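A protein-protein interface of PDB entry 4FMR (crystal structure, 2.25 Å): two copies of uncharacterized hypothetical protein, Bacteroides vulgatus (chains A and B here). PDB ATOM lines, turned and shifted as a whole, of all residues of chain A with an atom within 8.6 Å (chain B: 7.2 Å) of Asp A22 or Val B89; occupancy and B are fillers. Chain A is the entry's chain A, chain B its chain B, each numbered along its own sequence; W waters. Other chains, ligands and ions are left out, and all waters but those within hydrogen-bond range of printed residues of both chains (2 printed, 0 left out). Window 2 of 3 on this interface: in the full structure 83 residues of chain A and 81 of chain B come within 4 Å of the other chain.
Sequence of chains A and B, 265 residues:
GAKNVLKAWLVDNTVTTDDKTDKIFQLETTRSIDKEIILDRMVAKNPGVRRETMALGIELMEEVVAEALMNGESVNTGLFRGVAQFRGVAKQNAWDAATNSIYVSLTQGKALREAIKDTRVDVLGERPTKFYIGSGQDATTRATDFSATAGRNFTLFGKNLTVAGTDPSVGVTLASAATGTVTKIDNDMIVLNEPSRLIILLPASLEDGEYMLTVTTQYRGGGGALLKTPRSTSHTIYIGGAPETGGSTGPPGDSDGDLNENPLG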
ATOM      1  N   LEU A  10     -23.267 -17.840  -2.119  1.00  0.00           N
ATOM      2  CA  LEU A  10     -21.858 -17.484  -2.075  1.00  0.00           C
ATOM      3  C   LEU A  10     -21.285 -17.853  -3.434  1.00  0.00           C
ATOM      4  O   LEU A  10     -21.446 -19.006  -3.848  1.00  0.00           O
ATOM      5  CB  LEU A  10     -21.124 -18.197  -0.916  1.00  0.00           C
ATOM      6  CG  LEU A  10     -21.584 -17.865   0.495  1.00  0.00           C
ATOM      7  CD1 LEU A  10     -21.089 -18.888   1.460  1.00  0.00           C
ATOM      8  CD2 LEU A  10     -21.138 -16.490   0.913  1.00  0.00           C
ATOM      9  N   VAL A  11     -20.743 -16.862  -4.178  1.00  0.00           N
ATOM     10  CA  VAL A  11     -20.129 -17.015  -5.518  1.00  0.00           C
ATOM     11  C   VAL A  11     -18.734 -16.366  -5.510  1.00  0.00           C
ATOM     12  O   VAL A  11     -18.477 -15.456  -4.707  1.00  0.00           O
ATOM     13  CB  VAL A  11     -20.972 -16.482  -6.737  1.00  0.00           C
ATOM     14  CG1 VAL A  11     -22.320 -17.169  -6.842  1.00  0.00           C
ATOM     15  CG2 VAL A  11     -21.140 -14.965  -6.720  1.00  0.00           C
ATOM     16  N   ASP A  12     -17.858 -16.816  -6.430  1.00  0.00           N
ATOM     17  CA  ASP A  12     -16.503 -16.284  -6.623  1.00  0.00           C
ATOM     18  C   ASP A  12     -16.586 -14.936  -7.329  1.00  0.00           C
ATOM     19  O   ASP A  12     -17.453 -14.744  -8.185  1.00  0.00           O
ATOM     20  CB  ASP A  12     -15.626 -17.271  -7.416  1.00  0.00           C
ATOM     21  CG  ASP A  12     -15.337 -18.581  -6.707  1.00  0.00           C
ATOM     22  OD1 ASP A  12     -15.097 -18.554  -5.484  1.00  0.00           O
ATOM     23  OD2 ASP A  12     -15.267 -19.626  -7.392  1.00  0.00           O
ATOM     24  N   ASN A  13     -15.706 -13.995  -6.935  1.00  0.00           N
ATOM     25  CA  ASN A  13     -15.629 -12.609  -7.414  1.00  0.00           C
ATOM     26  C   ASN A  13     -14.733 -12.482  -8.655  1.00  0.00           C
ATOM     27  O   ASN A  13     -14.862 -13.244  -9.610  1.00  0.00           O
ATOM     28  CB  ASN A  13     -15.081 -11.735  -6.275  1.00  0.00           C
ATOM     29  CG  ASN A  13     -15.041 -10.244  -6.496  1.00  0.00           C
ATOM     30  OD1 ASN A  13     -15.651  -9.683  -7.416  1.00  0.00           O
ATOM     31  ND2 ASN A  13     -14.350  -9.560  -5.603  1.00  0.00           N
ATOM     32  N   THR A  21      -9.207 -15.283  -5.832  1.00  0.00           N
ATOM     33  CA  THR A  21     -10.379 -14.386  -5.784  1.00  0.00           C
ATOM     34  C   THR A  21     -11.194 -14.506  -4.460  1.00  0.00           C
ATOM     35  O   THR A  21     -11.072 -15.485  -3.719  1.00  0.00           O
ATOM     36  CB  THR A  21     -11.328 -14.632  -6.991  1.00  0.00           C
ATOM     37  OG1 THR A  21     -12.305 -13.592  -7.027  1.00  0.00           O
ATOM     38  CG2 THR A  21     -12.028 -16.004  -6.954  1.00  0.00           C
ATOM     39  N   ASP A  22     -12.035 -13.486  -4.210  1.00  0.00           N
ATOM     40  CA  ASP A  22     -12.954 -13.331  -3.072  1.00  0.00           C
ATOM     41  C   ASP A  22     -14.295 -14.059  -3.245  1.00  0.00           C
ATOM     42  O   ASP A  22     -14.718 -14.301  -4.376  1.00  0.00           O
ATOM     43  CB  ASP A  22     -13.309 -11.825  -2.928  1.00  0.00           C
ATOM     44  CG  ASP A  22     -12.365 -10.959  -2.132  1.00  0.00           C
ATOM     45  OD1 ASP A  22     -11.969 -11.379  -1.020  1.00  0.00           O
ATOM     46  OD2 ASP A  22     -12.136  -9.792  -2.551  1.00  0.00           O
ATOM     47  N   LYS A  23     -15.005 -14.310  -2.129  1.00  0.00           N
ATOM     48  CA  LYS A  23     -16.397 -14.760  -2.134  1.00  0.00           C
ATOM     49  C   LYS A  23     -17.270 -13.517  -1.984  1.00  0.00           C
ATOM     50  O   LYS A  23     -16.893 -12.582  -1.267  1.00  0.00           O
ATOM     51  CB  LYS A  23     -16.713 -15.807  -1.037  1.00  0.00           C
ATOM     52  CG  LYS A  23     -16.153 -17.206  -1.279  1.00  0.00           C
ATOM     53  CD  LYS A  23     -16.918 -17.983  -2.339  1.00  0.00           C
ATOM     54  CE  LYS A  23     -16.336 -19.363  -2.546  1.00  0.00           C
ATOM     55  NZ  LYS A  23     -16.971 -20.042  -3.706  1.00  0.00           N
ATOM     56  N   ILE A  24     -18.417 -13.493  -2.665  1.00  0.00           N
ATOM     57  CA  ILE A  24     -19.375 -12.388  -2.609  1.00  0.00           C
ATOM     58  C   ILE A  24     -20.787 -12.958  -2.565  1.00  0.00           C
ATOM     59  O   ILE A  24     -21.026 -14.098  -2.980  1.00  0.00           O
ATOM     60  CB  ILE A  24     -19.218 -11.345  -3.767  1.00  0.00           C
ATOM     61  CG1 ILE A  24     -19.222 -12.015  -5.154  1.00  0.00           C
ATOM     62  CG2 ILE A  24     -17.959 -10.447  -3.573  1.00  0.00           C
ATOM     63  CD1 ILE A  24     -20.074 -11.363  -6.074  1.00  0.00           C
ATOM     64  N   PHE A  25     -21.729 -12.150  -2.059  1.00  0.00           N
ATOM     65  CA  PHE A  25     -23.109 -12.571  -1.980  1.00  0.00           C
ATOM     66  C   PHE A  25     -23.832 -12.266  -3.273  1.00  0.00           C
ATOM     67  O   PHE A  25     -23.656 -11.197  -3.870  1.00  0.00           O
ATOM     68  CB  PHE A  25     -23.821 -11.913  -0.798  1.00  0.00           C
ATOM     69  CG  PHE A  25     -23.125 -12.198   0.499  1.00  0.00           C
ATOM     70  CD1 PHE A  25     -23.284 -13.425   1.139  1.00  0.00           C
ATOM     71  CD2 PHE A  25     -22.286 -11.251   1.079  1.00  0.00           C
ATOM     72  CE1 PHE A  25     -22.610 -13.696   2.332  1.00  0.00           C
ATOM     73  CE2 PHE A  25     -21.621 -11.524   2.278  1.00  0.00           C
ATOM     74  CZ  PHE A  25     -21.798 -12.737   2.901  1.00  0.00           C
ATOM     75  N   TYR A 132     -22.787 -22.024 -12.873  1.00  0.00           N
ATOM     76  CA  TYR A 132     -23.669 -20.903 -12.582  1.00  0.00           C
ATOM     77  C   TYR A 132     -23.256 -19.630 -13.298  1.00  0.00           C
ATOM     78  O   TYR A 132     -22.137 -19.519 -13.790  1.00  0.00           O
ATOM     79  CB  TYR A 132     -23.706 -20.628 -11.050  1.00  0.00           C
ATOM     80  CG  TYR A 132     -22.359 -20.311 -10.420  1.00  0.00           C
ATOM     81  CD1 TYR A 132     -21.844 -19.015 -10.441  1.00  0.00           C
ATOM     82  CD2 TYR A 132     -21.640 -21.287  -9.731  1.00  0.00           C
ATOM     83  CE1 TYR A 132     -20.623 -18.710  -9.839  1.00  0.00           C
ATOM     84  CE2 TYR A 132     -20.431 -20.986  -9.098  1.00  0.00           C
ATOM     85  CZ  TYR A 132     -19.928 -19.693  -9.152  1.00  0.00           C
ATOM     86  OH  TYR A 132     -18.733 -19.381  -8.545  1.00  0.00           O
ATOM     87  N   ARG B  87     -23.079  -5.350  -1.025  1.00  0.00           N
ATOM     88  CA  ARG B  87     -21.736  -4.758  -1.065  1.00  0.00           C
ATOM     89  C   ARG B  87     -20.834  -5.519  -0.122  1.00  0.00           C
ATOM     90  O   ARG B  87     -21.301  -6.066   0.879  1.00  0.00           O
ATOM     91  CB  ARG B  87     -21.717  -3.265  -0.711  1.00  0.00           C
ATOM     92  CG  ARG B  87     -22.445  -2.334  -1.656  1.00  0.00           C
ATOM     93  CD  ARG B  87     -22.091  -0.882  -1.364  1.00  0.00           C
ATOM     94  NE  ARG B  87     -23.214   0.043  -1.574  1.00  0.00           N
ATOM     95  CZ  ARG B  87     -23.515   0.622  -2.733  1.00  0.00           C
ATOM     96  NH1 ARG B  87     -22.805   0.355  -3.823  1.00  0.00           N
ATOM     97  NH2 ARG B  87     -24.554   1.440  -2.822  1.00  0.00           N
ATOM     98  N   GLY B  88     -19.549  -5.543  -0.446  1.00  0.00           N
ATOM     99  CA  GLY B  88     -18.535  -6.167   0.381  1.00  0.00           C
ATOM    100  C   GLY B  88     -18.358  -7.646   0.175  1.00  0.00           C
ATOM    101  O   GLY B  88     -19.241  -8.341  -0.333  1.00  0.00           O
ATOM    102  N   VAL B  89     -17.196  -8.111   0.609  1.00  0.00           N
ATOM    103  CA  VAL B  89     -16.699  -9.488   0.581  1.00  0.00           C
ATOM    104  C   VAL B  89     -17.411 -10.340   1.651  1.00  0.00           C
ATOM    105  O   VAL B  89     -17.712  -9.841   2.746  1.00  0.00           O
ATOM    106  CB  VAL B  89     -15.148  -9.442   0.841  1.00  0.00           C
ATOM    107  CG1 VAL B  89     -14.538 -10.830   1.004  1.00  0.00           C
ATOM    108  CG2 VAL B  89     -14.424  -8.668  -0.254  1.00  0.00           C
ATOM    109  N   ALA B  90     -17.615 -11.639   1.345  1.00  0.00           N
ATOM    110  CA  ALA B  90     -18.094 -12.616   2.307  1.00  0.00           C
ATOM    111  C   ALA B  90     -16.910 -13.077   3.205  1.00  0.00           C
ATOM    112  O   ALA B  90     -15.992 -13.784   2.741  1.00  0.00           O
ATOM    113  CB  ALA B  90     -18.729 -13.792   1.591  1.00  0.00           C
ATOM    114  N   LYS B  91     -16.897 -12.620   4.469  1.00  0.00           N
ATOM    115  CA  LYS B  91     -15.871 -13.006   5.447  1.00  0.00           C
ATOM    116  C   LYS B  91     -16.380 -14.203   6.222  1.00  0.00           C
ATOM    117  O   LYS B  91     -17.464 -14.148   6.812  1.00  0.00           O
ATOM    118  CB  LYS B  91     -15.505 -11.841   6.387  1.00  0.00           C
ATOM    119  CG  LYS B  91     -14.854 -10.658   5.678  1.00  0.00           C
ATOM    120  CD  LYS B  91     -14.614  -9.506   6.621  1.00  0.00           C
ATOM    121  CE  LYS B  91     -13.825  -8.406   5.959  1.00  0.00           C
ATOM    122  NZ  LYS B  91     -13.453  -7.330   6.918  1.00  0.00           N
ATOM    123  N   GLN B  92     -15.628 -15.313   6.160  1.00  0.00           N
ATOM    124  CA  GLN B  92     -15.934 -16.592   6.816  1.00  0.00           C
ATOM    125  C   GLN B  92     -17.302 -17.137   6.344  1.00  0.00           C
ATOM    126  O   GLN B  92     -18.048 -17.731   7.136  1.00  0.00           O
ATOM    127  CB  GLN B  92     -15.877 -16.470   8.358  1.00  0.00           C
ATOM    128  CG  GLN B  92     -14.486 -16.160   8.898  1.00  0.00           C
ATOM    129  CD  GLN B  92     -14.487 -15.875  10.381  1.00  0.00           C
ATOM    130  OE1 GLN B  92     -13.976 -14.843  10.830  1.00  0.00           O
ATOM    131  NE2 GLN B  92     -15.058 -16.781  11.175  1.00  0.00           N
ATOM    132  N   ALA B  94     -20.136 -15.845   5.727  1.00  0.00           N
ATOM    133  CA  ALA B  94     -21.248 -15.348   6.529  1.00  0.00           C
ATOM    134  C   ALA B  94     -21.380 -13.856   6.410  1.00  0.00           C
ATOM    135  O   ALA B  94     -20.387 -13.131   6.291  1.00  0.00           O
ATOM    136  CB  ALA B  94     -21.066 -15.735   7.999  1.00  0.00           C
ATOM    137  N   TRP B  95     -22.624 -13.396   6.456  1.00  0.00           N
ATOM    138  CA  TRP B  95     -22.937 -11.991   6.400  1.00  0.00           C
ATOM    139  C   TRP B  95     -22.395 -11.300   7.674  1.00  0.00           C
ATOM    140  O   TRP B  95     -22.619 -11.772   8.791  1.00  0.00           O
ATOM    141  CB  TRP B  95     -24.457 -11.809   6.241  1.00  0.00           C
ATOM    142  CG  TRP B  95     -24.878 -10.377   6.110  1.00  0.00           C
ATOM    143  CD1 TRP B  95     -25.187  -9.515   7.119  1.00  0.00           C
ATOM    144  CD2 TRP B  95     -25.008  -9.634   4.889  1.00  0.00           C
ATOM    145  NE1 TRP B  95     -25.499  -8.275   6.603  1.00  0.00           N
ATOM    146  CE2 TRP B  95     -25.416  -8.328   5.234  1.00  0.00           C
ATOM    147  CE3 TRP B  95     -24.774  -9.935   3.535  1.00  0.00           C
ATOM    148  CZ2 TRP B  95     -25.632  -7.336   4.272  1.00  0.00           C
ATOM    149  CZ3 TRP B  95     -24.984  -8.952   2.583  1.00  0.00           C
ATOM    150  CH2 TRP B  95     -25.443  -7.682   2.948  1.00  0.00           C
ATOM    151  N   ASP B  96     -21.637 -10.229   7.476  1.00  0.00           N
ATOM    152  CA  ASP B  96     -21.076  -9.383   8.520  1.00  0.00           C
ATOM    153  C   ASP B  96     -21.656  -7.981   8.345  1.00  0.00           C
ATOM    154  O   ASP B  96     -21.262  -7.267   7.421  1.00  0.00           O
ATOM    155  CB  ASP B  96     -19.535  -9.383   8.458  1.00  0.00           C
ATOM    156  CG  ASP B  96     -18.827  -8.565   9.527  1.00  0.00           C
ATOM    157  OD1 ASP B  96     -19.411  -8.368  10.616  1.00  0.00           O
ATOM    158  OD2 ASP B  96     -17.665  -8.179   9.302  1.00  0.00           O
ATOM    159  N   THR B  99     -19.395  -4.931   7.602  1.00  0.00           N
ATOM    160  CA  THR B  99     -18.655  -4.808   6.341  1.00  0.00           C
ATOM    161  C   THR B  99     -19.579  -4.990   5.136  1.00  0.00           C
ATOM    162  O   THR B  99     -19.264  -4.472   4.061  1.00  0.00           O
ATOM    163  CB  THR B  99     -17.475  -5.792   6.274  1.00  0.00           C
ATOM    164  OG1 THR B  99     -17.949  -7.132   6.405  1.00  0.00           O
ATOM    165  CG2 THR B  99     -16.407  -5.500   7.330  1.00  0.00           C
ATOM    166  N   ASN B 100     -20.706  -5.690   5.301  1.00  0.00           N
ATOM    167  CA  ASN B 100     -21.662  -5.907   4.216  1.00  0.00           C
ATOM    168  C   ASN B 100     -22.874  -5.040   4.368  1.00  0.00           C
ATOM    169  O   ASN B 100     -23.305  -4.749   5.488  1.00  0.00           O
ATOM    170  CB  ASN B 100     -22.091  -7.376   4.151  1.00  0.00           C
ATOM    171  CG  ASN B 100     -20.966  -8.358   3.987  1.00  0.00           C
ATOM    172  OD1 ASN B 100     -20.747  -9.212   4.856  1.00  0.00           O
ATOM    173  ND2 ASN B 100     -20.248  -8.275   2.861  1.00  0.00           N
HETATM  174  O   HOH W   1     -14.078 -14.535   0.858  1.00  0.00           O
HETATM  175  O   HOH W   2     -21.180  -9.236  -1.780  1.00  0.00           O
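The backbone NH (N) of Ala B90 is in hydrogen-bond range of the backbone carbonyl oxygen (O) of Lys A23 (2.9 Å).
The side-chain amino group (NZ) of Lys A23 is in salt-bridge range of the side-chain carboxylate (OD1) of Asp A12, 3.0 Å away.
O of Asp A22 is in hydrogen-bond range of N of Asn A13, at 2.8 Å.
O of Arg B87 is in hydrogen-bond range of ND2 of Asn B100 (3.1 Å).
ND2 of Asn B100 sits close to O of Gly B88, 3.3 Å away.
O of Val B89 lies within hydrogen-bond range of ND2 of Asn B100, 3.0 Å away.
N of Asp B96 lies within hydrogen-bond range of OD1 of Asn B100, 2.9 Å away.
Leu A10 touches Ala B90 (CD2 to CB, 3.7 Å).
Val B89 touches Asp A22 (CG1 to OD1, 3.3 Å).
CA of Val B89 touches O of Lys A23, 3.6 Å away.
CB of Ala B90 touches CZ of Phe A25 (3.5 Å).
O of Ala B94 touches CZ of Phe A25 (3.7 Å).
Trp B95 touches Phe A25 (N to CZ, 3.7 Å).
CE2 of Phe A25 touches OD1 of Asn B100, 3.6 Å away.
Of chain B, only Val B89 (3.3 Å) comes within 4 Å of Asp A22.
Printed residues of chain A within 4 Å of Val B89: Asp A22 (3.3 Å) and Lys A23 (3.6 Å).
No residue of chain A comes within 4 Å of Gly B88.
Of chain A, only Leu A10 (3.7 Å), Lys A23 (2.9 Å) and Phe A25 (3.5 Å) come within 4 Å of Ala B90.
Of the printed residues of chain B, Leu A10 touches Ala B90.
Printed residues of chain B within 4 Å of Phe A25: Ala B90 (3.5 Å), Ala B94 (3.7 Å), Trp B95 (3.7 Å) and Asn B100 (3.6 Å).
Printed residues of chain A within 4 Å of Ala B94: Phe A25 (3.7 Å).
Of the printed residues of chain A, Asn B100 touches Phe A25 (3.6 Å).
Of the printed residues of chain A, Trp B95 touches Phe A25 (3.7 Å).
Of the 11 printed residues of chain B, 5 touch a printed residue of chain A.
Hydrophobic or aromatic side chains of chain B that line the printed part of chain A: Val B89, Ala B90 and Trp B95.
Along chain B the printed residues that touch a printed residue of chain A span positions 89 to 100.
Hydrophobic or aromatic side chains of chain A within 4 Å of the printed part of chain B: Leu A10 and Phe A25.
Along chain A the printed residues that touch a printed residue of chain B span positions 10 to 25.
Among the printed residues, 8 pairs touch across the chains.
Among the printed residues, no Asp or Glu carboxylate lies within 4 Å of a Lys or Arg side-chain nitrogen of the other chain.
No position is printed for both chains.
Of the 8 pairs that touch across the chains among the printed residues, none has its exchanged pair printed and touching as well.
Water W2 lies within hydrogen-bond range of the backbone carbonyl oxygen (O) of Gly B88 (2.6 Å) and the backbone NH (N) of Phe A25 (3.0 Å).
Water W1 bridges O of Ala B90 and N of Lys A23.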
